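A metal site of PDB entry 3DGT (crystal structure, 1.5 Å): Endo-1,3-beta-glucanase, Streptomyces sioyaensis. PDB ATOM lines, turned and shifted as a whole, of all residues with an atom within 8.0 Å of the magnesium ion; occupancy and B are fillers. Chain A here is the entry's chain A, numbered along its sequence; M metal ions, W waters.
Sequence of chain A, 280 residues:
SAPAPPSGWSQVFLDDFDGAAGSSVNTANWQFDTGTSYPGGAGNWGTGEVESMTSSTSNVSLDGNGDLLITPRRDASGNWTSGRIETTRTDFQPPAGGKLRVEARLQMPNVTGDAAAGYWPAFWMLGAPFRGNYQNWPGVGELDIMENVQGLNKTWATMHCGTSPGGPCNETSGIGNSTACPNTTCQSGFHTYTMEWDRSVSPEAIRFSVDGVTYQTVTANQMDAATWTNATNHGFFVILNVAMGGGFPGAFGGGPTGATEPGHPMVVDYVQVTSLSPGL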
ATOM      1  N   SER A   1      15.285 -18.460 -11.082  1.00  0.00           N
ATOM      2  CA  SER A   1      14.273 -17.427 -10.704  1.00  0.00           C
ATOM      3  C   SER A   1      13.268 -17.203 -11.815  1.00  0.00           C
ATOM      4  O   SER A   1      13.594 -17.393 -12.995  1.00  0.00           O
ATOM      5  CB  SER A   1      14.951 -16.100 -10.395  1.00  0.00           C
ATOM      6  OG  SER A   1      15.909 -16.237  -9.359  1.00  0.00           O
ATOM      7  N   ALA A   2      12.061 -16.798 -11.440  1.00  0.00           N
ATOM      8  CA  ALA A   2      11.034 -16.461 -12.424  1.00  0.00           C
ATOM      9  C   ALA A   2      11.513 -15.304 -13.291  1.00  0.00           C
ATOM     10  O   ALA A   2      12.078 -14.331 -12.763  1.00  0.00           O
ATOM     11  CB  ALA A   2       9.712 -16.113 -11.743  1.00  0.00           C
ATOM     12  N   LEU A  14       4.177 -14.847  -5.925  1.00  0.00           N
ATOM     13  CA  LEU A  14       5.446 -15.447  -6.338  1.00  0.00           C
ATOM     14  C   LEU A  14       6.198 -15.932  -5.127  1.00  0.00           C
ATOM     15  O   LEU A  14       6.504 -15.164  -4.229  1.00  0.00           O
ATOM     16  CB  LEU A  14       6.310 -14.458  -7.136  1.00  0.00           C
ATOM     17  CG  LEU A  14       7.735 -14.954  -7.482  1.00  0.00           C
ATOM     18  CD1 LEU A  14       7.707 -16.131  -8.456  1.00  0.00           C
ATOM     19  CD2 LEU A  14       8.555 -13.819  -8.067  1.00  0.00           C
ATOM     20  N   ASP A  15       6.502 -17.224  -5.099  1.00  0.00           N
ATOM     21  CA  ASP A  15       7.513 -17.731  -4.174  1.00  0.00           C
ATOM     22  C   ASP A  15       8.589 -18.372  -5.006  1.00  0.00           C
ATOM     23  O   ASP A  15       8.344 -19.369  -5.692  1.00  0.00           O
ATOM     24  CB  ASP A  15       6.933 -18.743  -3.179  1.00  0.00           C
ATOM     25  CG  ASP A  15       7.865 -19.023  -2.005  1.00  0.00           C
ATOM     26  OD1 ASP A  15       9.089 -18.805  -2.128  1.00  0.00           O
ATOM     27  OD2 ASP A  15       7.352 -19.461  -0.960  1.00  0.00           O
ATOM     28  N   ASP A  16       9.771 -17.762  -4.958  1.00  0.00           N
ATOM     29  CA  ASP A  16      10.919 -18.236  -5.715  1.00  0.00           C
ATOM     30  C   ASP A  16      11.873 -19.091  -4.871  1.00  0.00           C
ATOM     31  O   ASP A  16      12.956 -19.478  -5.344  1.00  0.00           O
ATOM     32  CB  ASP A  16      11.651 -17.063  -6.387  1.00  0.00           C
ATOM     33  CG  ASP A  16      11.983 -17.331  -7.843  1.00  0.00           C
ATOM     34  OD1 ASP A  16      12.486 -18.427  -8.139  1.00  0.00           O
ATOM     35  OD2 ASP A  16      11.729 -16.444  -8.693  1.00  0.00           O
ATOM     36  N   PHE A  17      11.474 -19.422  -3.632  1.00  0.00           N
ATOM     37  CA  PHE A  17      12.175 -20.424  -2.816  1.00  0.00           C
ATOM     38  C   PHE A  17      13.641 -20.100  -2.584  1.00  0.00           C
ATOM     39  O   PHE A  17      14.482 -20.990  -2.528  1.00  0.00           O
ATOM     40  CB  PHE A  17      11.977 -21.835  -3.404  1.00  0.00           C
ATOM     41  CG  PHE A  17      10.541 -22.261  -3.457  1.00  0.00           C
ATOM     42  CD1 PHE A  17       9.811 -22.437  -2.281  1.00  0.00           C
ATOM     43  CD2 PHE A  17       9.922 -22.540  -4.671  1.00  0.00           C
ATOM     44  CE1 PHE A  17       8.495 -22.849  -2.310  1.00  0.00           C
ATOM     45  CE2 PHE A  17       8.580 -22.954  -4.720  1.00  0.00           C
ATOM     46  CZ  PHE A  17       7.861 -23.103  -3.520  1.00  0.00           C
ATOM     47  N   ASP A  18      13.941 -18.815  -2.430  1.00  0.00           N
ATOM     48  CA  ASP A  18      15.276 -18.375  -2.081  1.00  0.00           C
ATOM     49  C   ASP A  18      15.463 -18.497  -0.581  1.00  0.00           C
ATOM     50  O   ASP A  18      14.512 -18.389   0.192  1.00  0.00           O
ATOM     51  CB  ASP A  18      15.526 -16.938  -2.570  1.00  0.00           C
ATOM     52  CG  ASP A  18      15.452 -16.826  -4.083  1.00  0.00           C
ATOM     53  OD1 ASP A  18      16.089 -17.659  -4.785  1.00  0.00           O
ATOM     54  OD2 ASP A  18      14.754 -15.903  -4.571  1.00  0.00           O
ATOM     55  N   GLY A  19      16.702 -18.735  -0.186  1.00  0.00           N
ATOM     56  CA  GLY A  19      17.046 -18.983   1.220  1.00  0.00           C
ATOM     57  C   GLY A  19      18.116 -20.047   1.339  1.00  0.00           C
ATOM     58  O   GLY A  19      18.446 -20.716   0.351  1.00  0.00           O
ATOM     59  N   ASP A  63      17.204 -25.754  -1.374  1.00  0.00           N
ATOM     60  CA  ASP A  63      18.542 -26.190  -1.779  1.00  0.00           C
ATOM     61  C   ASP A  63      19.648 -25.136  -1.656  1.00  0.00           C
ATOM     62  O   ASP A  63      20.825 -25.453  -1.860  1.00  0.00           O
ATOM     63  CB  ASP A  63      18.536 -26.852  -3.175  1.00  0.00           C
ATOM     64  CG  ASP A  63      18.247 -25.874  -4.327  1.00  0.00           C
ATOM     65  OD1 ASP A  63      18.056 -24.675  -4.108  1.00  0.00           O
ATOM     66  OD2 ASP A  63      18.220 -26.342  -5.487  1.00  0.00           O
ATOM     67  N   ASN A  65      19.957 -22.656  -3.627  1.00  0.00           N
ATOM     68  CA  ASN A  65      20.227 -22.154  -4.971  1.00  0.00           C
ATOM     69  C   ASN A  65      18.976 -21.622  -5.642  1.00  0.00           C
ATOM     70  O   ASN A  65      18.957 -21.408  -6.847  1.00  0.00           O
ATOM     71  CB  ASN A  65      20.888 -23.237  -5.842  1.00  0.00           C
ATOM     72  CG  ASN A  65      22.225 -23.699  -5.279  1.00  0.00           C
ATOM     73  OD1 ASN A  65      22.924 -22.933  -4.618  1.00  0.00           O
ATOM     74  ND2 ASN A  65      22.577 -24.945  -5.541  1.00  0.00           N
ATOM     75  N   GLY A  66      17.948 -21.376  -4.833  1.00  0.00           N
ATOM     76  CA  GLY A  66      16.692 -20.811  -5.335  1.00  0.00           C
ATOM     77  C   GLY A  66      15.601 -21.837  -5.588  1.00  0.00           C
ATOM     78  O   GLY A  66      14.635 -21.548  -6.293  1.00  0.00           O
ATOM     79  N   ASP A  67      15.740 -23.034  -5.025  1.00  0.00           N
ATOM     80  CA  ASP A  67      14.762 -24.085  -5.265  1.00  0.00           C
ATOM     81  C   ASP A  67      14.257 -24.751  -4.002  1.00  0.00           C
ATOM     82  O   ASP A  67      15.004 -24.931  -3.027  1.00  0.00           O
ATOM     83  CB  ASP A  67      15.313 -25.199  -6.163  1.00  0.00           C
ATOM     84  CG  ASP A  67      16.077 -24.676  -7.351  1.00  0.00           C
ATOM     85  OD1 ASP A  67      15.468 -24.015  -8.214  1.00  0.00           O
ATOM     86  OD2 ASP A  67      17.291 -24.972  -7.440  1.00  0.00           O
ATOM     87  N   LEU A  68      12.988 -25.130  -4.052  1.00  0.00           N
ATOM     88  CA  LEU A  68      12.398 -26.058  -3.104  1.00  0.00           C
ATOM     89  C   LEU A  68      12.778 -27.484  -3.494  1.00  0.00           C
ATOM     90  O   LEU A  68      12.785 -27.818  -4.690  1.00  0.00           O
ATOM     91  CB  LEU A  68      10.879 -25.930  -3.138  1.00  0.00           C
ATOM     92  CG  LEU A  68      10.046 -26.954  -2.373  1.00  0.00           C
ATOM     93  CD1 LEU A  68      10.147 -26.709  -0.893  1.00  0.00           C
ATOM     94  CD2 LEU A  68       8.604 -26.862  -2.823  1.00  0.00           C
ATOM     95  N   ARG A 105       8.220 -23.686 -12.305  1.00  0.00           N
ATOM     96  CA  ARG A 105       9.381 -24.168 -13.032  1.00  0.00           C
ATOM     97  C   ARG A 105      10.027 -25.193 -12.134  1.00  0.00           C
ATOM     98  O   ARG A 105      10.369 -24.891 -10.983  1.00  0.00           O
ATOM     99  CB  ARG A 105      10.335 -23.017 -13.369  1.00  0.00           C
ATOM    100  CG  ARG A 105      11.604 -23.443 -14.085  1.00  0.00           C
ATOM    101  CD  ARG A 105      12.381 -22.230 -14.570  1.00  0.00           C
ATOM    102  NE  ARG A 105      13.549 -22.601 -15.371  1.00  0.00           N
ATOM    103  CZ  ARG A 105      14.810 -22.542 -14.959  1.00  0.00           C
ATOM    104  NH1 ARG A 105      15.115 -22.119 -13.733  1.00  0.00           N
ATOM    105  NH2 ARG A 105      15.782 -22.916 -15.780  1.00  0.00           N
ATOM    106  N   PHE A 190      15.198 -28.317 -15.446  1.00  0.00           N
ATOM    107  CA  PHE A 190      14.012 -27.495 -15.311  1.00  0.00           C
ATOM    108  C   PHE A 190      13.161 -27.452 -16.559  1.00  0.00           C
ATOM    109  O   PHE A 190      13.666 -27.403 -17.679  1.00  0.00           O
ATOM    110  CB  PHE A 190      14.397 -26.069 -14.909  1.00  0.00           C
ATOM    111  CG  PHE A 190      14.947 -25.955 -13.518  1.00  0.00           C
ATOM    112  CD1 PHE A 190      14.147 -26.202 -12.416  1.00  0.00           C
ATOM    113  CD2 PHE A 190      16.270 -25.586 -13.322  1.00  0.00           C
ATOM    114  CE1 PHE A 190      14.664 -26.096 -11.121  1.00  0.00           C
ATOM    115  CE2 PHE A 190      16.795 -25.461 -12.036  1.00  0.00           C
ATOM    116  CZ  PHE A 190      15.982 -25.728 -10.933  1.00  0.00           C
ATOM    117  N   VAL A 268      11.954 -27.427  -7.332  1.00  0.00           N
ATOM    118  CA  VAL A 268      11.027 -26.379  -7.792  1.00  0.00           C
ATOM    119  C   VAL A 268      11.657 -25.002  -7.641  1.00  0.00           C
ATOM    120  O   VAL A 268      11.861 -24.532  -6.531  1.00  0.00           O
ATOM    121  CB  VAL A 268       9.688 -26.438  -7.015  1.00  0.00           C
ATOM    122  CG1 VAL A 268       8.666 -25.456  -7.618  1.00  0.00           C
ATOM    123  CG2 VAL A 268       9.136 -27.876  -6.976  1.00  0.00           C
ATOM    124  N   ASP A 269      11.936 -24.344  -8.768  1.00  0.00           N
ATOM    125  CA  ASP A 269      12.500 -22.992  -8.737  1.00  0.00           C
ATOM    126  C   ASP A 269      11.496 -21.960  -8.225  1.00  0.00           C
ATOM    127  O   ASP A 269      11.841 -21.111  -7.389  1.00  0.00           O
ATOM    128  CB  ASP A 269      13.002 -22.621 -10.133  1.00  0.00           C
ATOM    129  CG  ASP A 269      13.707 -21.273 -10.191  1.00  0.00           C
ATOM    130  OD1 ASP A 269      14.030 -20.672  -9.139  1.00  0.00           O
ATOM    131  OD2 ASP A 269      13.960 -20.822 -11.328  1.00  0.00           O
ATOM    132  N   TYR A 270      10.265 -22.043  -8.683  1.00  0.00           N
ATOM    133  CA  TYR A 270       9.255 -21.100  -8.252  1.00  0.00           C
ATOM    134  C   TYR A 270       7.853 -21.603  -8.540  1.00  0.00           C
ATOM    135  O   TYR A 270       7.659 -22.502  -9.355  1.00  0.00           O
ATOM    136  CB  TYR A 270       9.456 -19.719  -8.911  1.00  0.00           C
ATOM    137  CG  TYR A 270       9.238 -19.689 -10.409  1.00  0.00           C
ATOM    138  CD1 TYR A 270       7.948 -19.559 -10.950  1.00  0.00           C
ATOM    139  CD2 TYR A 270      10.311 -19.799 -11.295  1.00  0.00           C
ATOM    140  CE1 TYR A 270       7.748 -19.521 -12.333  1.00  0.00           C
ATOM    141  CE2 TYR A 270      10.112 -19.761 -12.678  1.00  0.00           C
ATOM    142  CZ  TYR A 270       8.826 -19.634 -13.174  1.00  0.00           C
ATOM    143  OH  TYR A 270       8.624 -19.599 -14.543  1.00  0.00           O
ATOM    144  N   VAL A 271       6.892 -21.002  -7.831  1.00  0.00           N
ATOM    145  CA  VAL A 271       5.484 -21.034  -8.181  1.00  0.00           C
ATOM    146  C   VAL A 271       5.051 -19.581  -8.324  1.00  0.00           C
ATOM    147  O   VAL A 271       5.357 -18.760  -7.472  1.00  0.00           O
ATOM    148  CB  VAL A 271       4.628 -21.756  -7.109  1.00  0.00           C
ATOM    149  CG1 VAL A 271       3.129 -21.568  -7.398  1.00  0.00           C
ATOM    150  CG2 VAL A 271       4.978 -23.238  -7.053  1.00  0.00           C
HETATM  151 MG    MG M   1      13.581 -19.962  -7.261  1.00  0.00          MG
HETATM  152  O   HOH W   1      15.173 -18.653  -7.156  1.00  0.00           O
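OD2 of Asp 16 sits at hydrogen-bond distance from N of Ala 2, 2.8 Å away.
The side-chain carboxylate (OD1) of Asp 63 is in hydrogen-bond range of the backbone NH (N) of Gly 66, at 3.4 Å.
OD2 of Asp 269 lies within hydrogen-bond range of N of Ser 1 (2.7 Å).
The side-chain carboxylate of Asp 269 lies within salt-bridge range of the guanidinium group of Arg 105 (3.0 Å).
The magnesium ion is bound by the side-chain carboxylate of Asp 269, water W1, the backbone carbonyl oxygen of Asp 16, the side-chain carboxylate of Asp 16, the backbone carbonyl oxygen of Asp 269 and the backbone carbonyl oxygen of Gly 66.
The magnesium ion has six donor atoms within binding distance.
Within 4 Å of the magnesium ion: Asp 16, Gly 66 and Asp 269.
The nearest printed residue that does not touch the magnesium ion is Tyr 270 (4.2 Å).
Water W1 lies within hydrogen-bond range of the side-chain carboxylate of Asp 18 and the side-chain hydroxyl of Ser 1.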
